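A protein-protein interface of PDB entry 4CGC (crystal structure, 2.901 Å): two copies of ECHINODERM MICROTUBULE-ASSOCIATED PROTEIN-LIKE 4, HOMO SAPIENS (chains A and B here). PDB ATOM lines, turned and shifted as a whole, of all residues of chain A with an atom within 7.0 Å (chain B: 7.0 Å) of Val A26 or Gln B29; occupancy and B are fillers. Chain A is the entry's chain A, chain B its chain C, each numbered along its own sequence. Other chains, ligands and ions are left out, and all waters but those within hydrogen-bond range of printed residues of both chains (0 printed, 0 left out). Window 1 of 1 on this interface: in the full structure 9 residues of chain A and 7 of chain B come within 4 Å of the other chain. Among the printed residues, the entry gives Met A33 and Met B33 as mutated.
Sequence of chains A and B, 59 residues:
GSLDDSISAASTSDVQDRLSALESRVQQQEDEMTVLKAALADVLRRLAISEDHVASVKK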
ATOM      1  N   ALA A  21       8.730   3.621 -29.936  1.00  0.00           N
ATOM      2  CA  ALA A  21       9.435   2.649 -29.113  1.00  0.00           C
ATOM      3  C   ALA A  21      10.795   3.198 -28.727  1.00  0.00           C
ATOM      4  O   ALA A  21      11.333   2.887 -27.667  1.00  0.00           O
ATOM      5  CB  ALA A  21       9.574   1.325 -29.839  1.00  0.00           C
ATOM      6  N   LEU A  22      11.347   4.034 -29.602  1.00  0.00           N
ATOM      7  CA  LEU A  22      12.635   4.669 -29.357  1.00  0.00           C
ATOM      8  C   LEU A  22      12.509   5.810 -28.351  1.00  0.00           C
ATOM      9  O   LEU A  22      13.344   5.947 -27.460  1.00  0.00           O
ATOM     10  CB  LEU A  22      13.239   5.178 -30.668  1.00  0.00           C
ATOM     11  CG  LEU A  22      14.164   4.213 -31.416  1.00  0.00           C
ATOM     12  CD1 LEU A  22      14.449   4.715 -32.824  1.00  0.00           C
ATOM     13  CD2 LEU A  22      15.456   3.996 -30.645  1.00  0.00           C
ATOM     14  N   GLU A  23      11.459   6.622 -28.486  1.00  0.00           N
ATOM     15  CA  GLU A  23      11.276   7.760 -27.590  1.00  0.00           C
ATOM     16  C   GLU A  23      10.896   7.276 -26.202  1.00  0.00           C
ATOM     17  O   GLU A  23      11.037   8.004 -25.218  1.00  0.00           O
ATOM     18  CB  GLU A  23      10.209   8.721 -28.117  1.00  0.00           C
ATOM     19  CG  GLU A  23      10.139   8.825 -29.617  1.00  0.00           C
ATOM     20  CD  GLU A  23       9.017   9.721 -30.094  1.00  0.00           C
ATOM     21  OE1 GLU A  23       7.875   9.225 -30.187  1.00  0.00           O
ATOM     22  OE2 GLU A  23       9.277  10.905 -30.400  1.00  0.00           O
ATOM     23  N   SER A  24      10.426   6.033 -26.128  1.00  0.00           N
ATOM     24  CA  SER A  24      10.112   5.402 -24.857  1.00  0.00           C
ATOM     25  C   SER A  24      11.404   4.972 -24.161  1.00  0.00           C
ATOM     26  O   SER A  24      11.622   5.261 -22.989  1.00  0.00           O
ATOM     27  CB  SER A  24       9.173   4.209 -25.064  1.00  0.00           C
ATOM     28  OG  SER A  24       8.795   3.640 -23.826  1.00  0.00           O
ATOM     29  N   ARG A  25      12.257   4.270 -24.904  1.00  0.00           N
ATOM     30  CA  ARG A  25      13.538   3.790 -24.389  1.00  0.00           C
ATOM     31  C   ARG A  25      14.409   4.949 -23.921  1.00  0.00           C
ATOM     32  O   ARG A  25      15.055   4.875 -22.881  1.00  0.00           O
ATOM     33  CB  ARG A  25      14.278   2.984 -25.467  1.00  0.00           C
ATOM     34  CG  ARG A  25      13.593   1.690 -25.854  1.00  0.00           C
ATOM     35  CD  ARG A  25      14.260   0.991 -27.045  1.00  0.00           C
ATOM     36  NE  ARG A  25      15.612   0.505 -26.766  1.00  0.00           N
ATOM     37  CZ  ARG A  25      16.411  -0.035 -27.680  1.00  0.00           C
ATOM     38  NH1 ARG A  25      15.991  -0.166 -28.931  1.00  0.00           N
ATOM     39  NH2 ARG A  25      17.623  -0.459 -27.348  1.00  0.00           N
ATOM     40  N   VAL A  26      14.389   6.036 -24.685  1.00  0.00           N
ATOM     41  CA  VAL A  26      15.242   7.181 -24.400  1.00  0.00           C
ATOM     42  C   VAL A  26      14.793   7.905 -23.129  1.00  0.00           C
ATOM     43  O   VAL A  26      15.626   8.295 -22.305  1.00  0.00           O
ATOM     44  CB  VAL A  26      15.249   8.162 -25.598  1.00  0.00           C
ATOM     45  CG1 VAL A  26      15.870   9.487 -25.216  1.00  0.00           C
ATOM     46  CG2 VAL A  26      15.994   7.550 -26.764  1.00  0.00           C
ATOM     47  N   GLN A  27      13.482   8.053 -22.952  1.00  0.00           N
ATOM     48  CA  GLN A  27      12.957   8.679 -21.744  1.00  0.00           C
ATOM     49  C   GLN A  27      13.280   7.827 -20.531  1.00  0.00           C
ATOM     50  O   GLN A  27      13.679   8.336 -19.487  1.00  0.00           O
ATOM     51  CB  GLN A  27      11.448   8.904 -21.849  1.00  0.00           C
ATOM     52  CG  GLN A  27      10.884   9.662 -20.666  1.00  0.00           C
ATOM     53  CD  GLN A  27      11.540  11.014 -20.482  1.00  0.00           C
ATOM     54  OE1 GLN A  27      11.463  11.875 -21.354  1.00  0.00           O
ATOM     55  NE2 GLN A  27      12.201  11.204 -19.345  1.00  0.00           N
ATOM     56  N   GLN A  28      13.128   6.519 -20.701  1.00  0.00           N
ATOM     57  CA  GLN A  28      13.416   5.539 -19.657  1.00  0.00           C
ATOM     58  C   GLN A  28      14.897   5.584 -19.330  1.00  0.00           C
ATOM     59  O   GLN A  28      15.304   5.462 -18.174  1.00  0.00           O
ATOM     60  CB  GLN A  28      12.997   4.136 -20.107  1.00  0.00           C
ATOM     61  CG  GLN A  28      13.554   2.971 -19.283  1.00  0.00           C
ATOM     62  CD  GLN A  28      13.090   2.961 -17.837  1.00  0.00           C
ATOM     63  OE1 GLN A  28      11.901   3.106 -17.553  1.00  0.00           O
ATOM     64  NE2 GLN A  28      14.024   2.750 -16.916  1.00  0.00           N
ATOM     65  N   GLN A  29      15.695   5.782 -20.374  1.00  0.00           N
ATOM     66  CA  GLN A  29      17.140   5.890 -20.238  1.00  0.00           C
ATOM     67  C   GLN A  29      17.520   7.174 -19.512  1.00  0.00           C
ATOM     68  O   GLN A  29      18.360   7.164 -18.610  1.00  0.00           O
ATOM     69  CB  GLN A  29      17.801   5.873 -21.621  1.00  0.00           C
ATOM     70  CG  GLN A  29      18.762   4.734 -21.864  1.00  0.00           C
ATOM     71  CD  GLN A  29      19.834   4.659 -20.810  1.00  0.00           C
ATOM     72  OE1 GLN A  29      19.826   3.756 -19.967  1.00  0.00           O
ATOM     73  NE2 GLN A  29      20.767   5.606 -20.846  1.00  0.00           N
ATOM     74  N   GLU A  30      16.846   8.267 -19.869  1.00  0.00           N
ATOM     75  CA  GLU A  30      17.056   9.548 -19.202  1.00  0.00           C
ATOM     76  C   GLU A  30      16.626   9.485 -17.741  1.00  0.00           C
ATOM     77  O   GLU A  30      17.297  10.031 -16.869  1.00  0.00           O
ATOM     78  CB  GLU A  30      16.320  10.689 -19.931  1.00  0.00           C
ATOM     79  CG  GLU A  30      16.162  11.951 -19.068  1.00  0.00           C
ATOM     80  CD  GLU A  30      16.181  13.253 -19.857  1.00  0.00           C
ATOM     81  OE1 GLU A  30      15.364  13.419 -20.794  1.00  0.00           O
ATOM     82  OE2 GLU A  30      17.025  14.118 -19.523  1.00  0.00           O
ATOM     83  N   ASP A  31      15.544   8.762 -17.469  1.00  0.00           N
ATOM     84  CA  ASP A  31      15.047   8.626 -16.101  1.00  0.00           C
ATOM     85  C   ASP A  31      16.033   7.851 -15.240  1.00  0.00           C
ATOM     86  O   ASP A  31      16.319   8.235 -14.107  1.00  0.00           O
ATOM     87  CB  ASP A  31      13.682   7.938 -16.089  1.00  0.00           C
ATOM     88  CG  ASP A  31      12.566   8.853 -16.546  1.00  0.00           C
ATOM     89  OD1 ASP A  31      12.743  10.093 -16.484  1.00  0.00           O
ATOM     90  OD2 ASP A  31      11.516   8.329 -16.976  1.00  0.00           O
ATOM     91  N   GLU A  32      16.556   6.759 -15.779  1.00  0.00           N
ATOM     92  CA  GLU A  32      17.573   5.981 -15.090  1.00  0.00           C
ATOM     93  C   GLU A  32      18.815   6.810 -14.692  1.00  0.00           C
ATOM     94  O   GLU A  32      19.384   6.600 -13.626  1.00  0.00           O
ATOM     95  CB  GLU A  32      17.995   4.794 -15.949  1.00  0.00           C
ATOM     96  CG  GLU A  32      17.974   3.483 -15.195  1.00  0.00           C
ATOM     97  CD  GLU A  32      17.362   2.351 -15.992  1.00  0.00           C
ATOM     98  OE1 GLU A  32      16.369   2.598 -16.704  1.00  0.00           O
ATOM     99  OE2 GLU A  32      17.871   1.214 -15.899  1.00  0.00           O
ATOM    100  N   MET A  33      19.218   7.741 -15.550  1.00  0.00           N
ATOM    101  CA  MET A  33      20.398   8.570 -15.262  1.00  0.00           C
ATOM    102  C   MET A  33      20.161   9.545 -14.133  1.00  0.00           C
ATOM    103  O   MET A  33      20.965   9.672 -13.216  1.00  0.00           O
ATOM    104  CB  MET A  33      20.851   9.333 -16.510  1.00  0.00           C
ATOM    105  CG  MET A  33      21.968   8.665 -17.318  1.00  0.00           C
ATOM    106  SD  MET A  33      23.657   8.475 -16.368  1.00  0.00           S
ATOM    107  CE  MET A  33      23.659  10.149 -15.381  1.00  0.00           C
ATOM    108  N   ALA B  21      15.300  15.081 -33.189  1.00  0.00           N
ATOM    109  CA  ALA B  21      15.184  15.353 -31.766  1.00  0.00           C
ATOM    110  C   ALA B  21      15.633  14.143 -30.965  1.00  0.00           C
ATOM    111  O   ALA B  21      16.161  14.271 -29.864  1.00  0.00           O
ATOM    112  CB  ALA B  21      13.766  15.740 -31.407  1.00  0.00           C
ATOM    113  N   LEU B  22      15.456  12.956 -31.543  1.00  0.00           N
ATOM    114  CA  LEU B  22      15.865  11.729 -30.872  1.00  0.00           C
ATOM    115  C   LEU B  22      17.375  11.575 -30.909  1.00  0.00           C
ATOM    116  O   LEU B  22      17.989  11.224 -29.902  1.00  0.00           O
ATOM    117  CB  LEU B  22      15.198  10.496 -31.498  1.00  0.00           C
ATOM    118  CG  LEU B  22      13.878  10.004 -30.891  1.00  0.00           C
ATOM    119  CD1 LEU B  22      13.202   8.959 -31.777  1.00  0.00           C
ATOM    120  CD2 LEU B  22      14.085   9.475 -29.479  1.00  0.00           C
ATOM    121  N   SER B  24      19.426  13.835 -31.034  1.00  0.00           N
ATOM    122  CA  SER B  24      19.946  14.875 -30.160  1.00  0.00           C
ATOM    123  C   SER B  24      19.927  14.401 -28.716  1.00  0.00           C
ATOM    124  O   SER B  24      20.931  14.482 -28.016  1.00  0.00           O
ATOM    125  CB  SER B  24      19.137  16.169 -30.314  1.00  0.00           C
ATOM    126  OG  SER B  24      19.678  17.212 -29.520  1.00  0.00           O
ATOM    127  N   ARG B  25      18.769  13.906 -28.285  1.00  0.00           N
ATOM    128  CA  ARG B  25      18.594  13.425 -26.921  1.00  0.00           C
ATOM    129  C   ARG B  25      19.561  12.283 -26.622  1.00  0.00           C
ATOM    130  O   ARG B  25      20.139  12.222 -25.535  1.00  0.00           O
ATOM    131  CB  ARG B  25      17.146  12.968 -26.694  1.00  0.00           C
ATOM    132  CG  ARG B  25      16.113  14.078 -26.757  1.00  0.00           C
ATOM    133  CD  ARG B  25      14.679  13.552 -26.682  1.00  0.00           C
ATOM    134  NE  ARG B  25      14.369  12.938 -25.395  1.00  0.00           N
ATOM    135  CZ  ARG B  25      13.229  12.313 -25.119  1.00  0.00           C
ATOM    136  NH1 ARG B  25      12.278  12.223 -26.040  1.00  0.00           N
ATOM    137  NH2 ARG B  25      13.031  11.794 -23.918  1.00  0.00           N
ATOM    138  N   VAL B  26      19.754  11.393 -27.597  1.00  0.00           N
ATOM    139  CA  VAL B  26      20.586  10.208 -27.388  1.00  0.00           C
ATOM    140  C   VAL B  26      22.056  10.587 -27.262  1.00  0.00           C
ATOM    141  O   VAL B  26      22.780  10.055 -26.421  1.00  0.00           O
ATOM    142  CB  VAL B  26      20.425   9.198 -28.540  1.00  0.00           C
ATOM    143  CG1 VAL B  26      21.477   8.101 -28.454  1.00  0.00           C
ATOM    144  CG2 VAL B  26      19.035   8.585 -28.516  1.00  0.00           C
ATOM    145  N   GLN B  27      22.490  11.536 -28.083  1.00  0.00           N
ATOM    146  CA  GLN B  27      23.871  11.999 -28.013  1.00  0.00           C
ATOM    147  C   GLN B  27      24.134  12.653 -26.665  1.00  0.00           C
ATOM    148  O   GLN B  27      25.187  12.450 -26.070  1.00  0.00           O
ATOM    149  CB  GLN B  27      24.203  12.963 -29.160  1.00  0.00           C
ATOM    150  CG  GLN B  27      25.677  13.386 -29.200  1.00  0.00           C
ATOM    151  CD  GLN B  27      26.643  12.209 -29.334  1.00  0.00           C
ATOM    152  OE1 GLN B  27      26.617  11.472 -30.321  1.00  0.00           O
ATOM    153  NE2 GLN B  27      27.501  12.039 -28.334  1.00  0.00           N
ATOM    154  N   GLN B  28      23.171  13.421 -26.170  1.00  0.00           N
ATOM    155  CA  GLN B  28      23.336  14.069 -24.874  1.00  0.00           C
ATOM    156  C   GLN B  28      23.440  13.018 -23.766  1.00  0.00           C
ATOM    157  O   GLN B  28      24.201  13.190 -22.819  1.00  0.00           O
ATOM    158  CB  GLN B  28      22.194  15.046 -24.581  1.00  0.00           C
ATOM    159  CG  GLN B  28      22.671  16.465 -24.280  1.00  0.00           C
ATOM    160  CD  GLN B  28      23.366  17.115 -25.467  1.00  0.00           C
ATOM    161  OE1 GLN B  28      22.846  17.115 -26.591  1.00  0.00           O
ATOM    162  NE2 GLN B  28      24.557  17.667 -25.233  1.00  0.00           N
ATOM    163  N   GLN B  29      22.669  11.937 -23.891  1.00  0.00           N
ATOM    164  CA  GLN B  29      22.760  10.821 -22.952  1.00  0.00           C
ATOM    165  C   GLN B  29      24.108  10.134 -23.062  1.00  0.00           C
ATOM    166  O   GLN B  29      24.706   9.749 -22.054  1.00  0.00           O
ATOM    167  CB  GLN B  29      21.656   9.799 -23.213  1.00  0.00           C
ATOM    168  CG  GLN B  29      20.310  10.165 -22.647  1.00  0.00           C
ATOM    169  CD  GLN B  29      19.199   9.316 -23.227  1.00  0.00           C
ATOM    170  OE1 GLN B  29      18.026   9.656 -23.112  1.00  0.00           O
ATOM    171  NE2 GLN B  29      19.566   8.206 -23.862  1.00  0.00           N
ATOM    172  N   GLU B  30      24.570   9.987 -24.293  1.00  0.00           N
ATOM    173  CA  GLU B  30      25.807   9.290 -24.584  1.00  0.00           C
ATOM    174  C   GLU B  30      26.941  10.037 -23.909  1.00  0.00           C
ATOM    175  O   GLU B  30      27.864   9.451 -23.336  1.00  0.00           O
ATOM    176  CB  GLU B  30      26.020   9.236 -26.094  1.00  0.00           C
ATOM    177  CG  GLU B  30      26.384   7.893 -26.663  1.00  0.00           C
ATOM    178  CD  GLU B  30      25.883   7.729 -28.086  1.00  0.00           C
ATOM    179  OE1 GLU B  30      26.211   8.581 -28.940  1.00  0.00           O
ATOM    180  OE2 GLU B  30      25.168   6.741 -28.352  1.00  0.00           O
ATOM    181  N   ASP B  31      26.817  11.357 -23.965  1.00  0.00           N
ATOM    182  CA  ASP B  31      27.756  12.280 -23.359  1.00  0.00           C
ATOM    183  C   ASP B  31      27.613  12.244 -21.839  1.00  0.00           C
ATOM    184  O   ASP B  31      28.607  12.197 -21.116  1.00  0.00           O
ATOM    185  CB  ASP B  31      27.516  13.689 -23.902  1.00  0.00           C
ATOM    186  CG  ASP B  31      27.948  13.829 -25.352  1.00  0.00           C
ATOM    187  OD1 ASP B  31      28.760  12.995 -25.812  1.00  0.00           O
ATOM    188  OD2 ASP B  31      27.464  14.762 -26.035  1.00  0.00           O
ATOM    189  N   GLU B  32      26.371  12.260 -21.364  1.00  0.00           N
ATOM    190  CA  GLU B  32      26.091  12.155 -19.935  1.00  0.00           C
ATOM    191  C   GLU B  32      26.749  10.902 -19.356  1.00  0.00           C
ATOM    192  O   GLU B  32      27.346  10.943 -18.280  1.00  0.00           O
ATOM    193  CB  GLU B  32      24.579  12.144 -19.673  1.00  0.00           C
ATOM    194  CG  GLU B  32      23.944  13.530 -19.598  1.00  0.00           C
ATOM    195  CD  GLU B  32      22.418  13.485 -19.584  1.00  0.00           C
ATOM    196  OE1 GLU B  32      21.849  12.519 -19.029  1.00  0.00           O
ATOM    197  OE2 GLU B  32      21.782  14.424 -20.113  1.00  0.00           O
ATOM    198  N   MET B  33      26.645   9.800 -20.093  1.00  0.00           N
ATOM    199  CA  MET B  33      27.251   8.529 -19.712  1.00  0.00           C
ATOM    200  C   MET B  33      28.767   8.578 -19.531  1.00  0.00           C
ATOM    201  O   MET B  33      29.289   8.221 -18.474  1.00  0.00           O
ATOM    202  CB  MET B  33      26.929   7.471 -20.760  1.00  0.00           C
ATOM    203  CG  MET B  33      26.247   6.240 -20.197  1.00  0.00           C
ATOM    204  SD  MET B  33      26.995   5.596 -18.529  1.00  0.00           S
ATOM    205  CE  MET B  33      25.333   4.953 -17.769  1.00  0.00           C
ATOM    206  N   THR B  34      29.475   8.971 -20.585  1.00  0.00           N
ATOM    207  CA  THR B  34      30.934   9.024 -20.547  1.00  0.00           C
ATOM    208  C   THR B  34      31.451   9.891 -19.396  1.00  0.00           C
ATOM    209  O   THR B  34      32.467   9.574 -18.775  1.00  0.00           O
ATOM    210  CB  THR B  34      31.530   9.523 -21.881  1.00  0.00           C
ATOM    211  OG1 THR B  34      31.213  10.913 -22.049  1.00  0.00           O
ATOM    212  CG2 THR B  34      30.963   8.747 -23.060  1.00  0.00           C
ATOM    213  N   VAL B  35      30.741  10.988 -19.114  1.00  0.00           N
ATOM    214  CA  VAL B  35      31.113  11.879 -18.020  1.00  0.00           C
ATOM    215  C   VAL B  35      31.052  11.167 -16.673  1.00  0.00           C
ATOM    216  O   VAL B  35      31.954  11.316 -15.837  1.00  0.00           O
ATOM    217  CB  VAL B  35      30.200  13.126 -17.996  1.00  0.00           C
ATOM    218  CG1 VAL B  35      30.449  13.966 -16.755  1.00  0.00           C
ATOM    219  CG2 VAL B  35      30.387  13.921 -19.272  1.00  0.00           C
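Of the 13 printed residues of chain A, 6 touch a printed residue of chain B. Printed residues of chain A that touch a printed residue of chain B: Leu A22, Glu A23, Val A26, Gln A27, Gln A29 and Glu A30. Of the 14 printed residues of chain B, 4 touch a printed residue of chain A. Hydrophobic or aromatic side chains of chain B that line the printed part of chain A: Leu B22 and Val B26. Among the printed residues, 9 pairs touch across the chains.
O of Val A26 lies close to OE1 of Gln B29, 2.9 Å away. OE1 of Gln A27 sits at hydrogen-bond distance from NH2 of Arg B25.
The side-chain amide nitrogen of Gln A27 sits at hydrogen-bond distance from the side-chain carboxylate of Asp A31, 3.1 Å away.
Leu A22 touches its own counterpart, Leu B22. Val A26 touches Gln B29, but with the chains exchanged Gln A29 does not touch Val B26 (7.4 Å). Gln A27 touches Arg B25, but with the chains exchanged Arg A25 does not touch Gln B27 (11.2 Å). Gln B29 touches its own counterpart, Gln A29. Positions printed for both chains: 21, 22, 24, 25, 26, 27, 28, 29, 30, 31, 32 and 33. Of the 9 pairs that touch across the chains among the printed residues, 3 have their exchanged pair printed and touching as well.
Of the printed residues of chain B, Val A26 touches Leu B22, Arg B25, Val B26 and Gln B29. Printed residues of chain A within 4 Å of Gln B29: Val A26 (2.9 Å), Gln A29 (3.7 Å) and Glu A30 (3.7 Å). Printed residues of chain A within 4 Å of Val B26: Val A26. Printed residues of chain A within 4 Å of Arg B25: Val A26 and Gln A27. Printed residues of chain B within 4 Å of Gln A29: Gln B29 (3.7 Å). Arg A25 touches none of the printed residues of chain B. Gln B28 touches none of the printed residues of chain A.
Leu A22 touches Leu B22 (CB to CD1, 3.9 Å). Glu A23 touches Leu B22 (CG to CD1, 3.8 Å). Leu B22 touches Val A26 (CD2 to CG2, 3.8 Å). Val A26 touches Arg B25. CG2 of Val B26 touches CG2 of Val A26 (3.7 Å). CB of Gln A29 touches NE2 of Gln B29, 3.7 Å away. Glu A30 touches Gln B29 (N to OE1, 3.7 Å).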
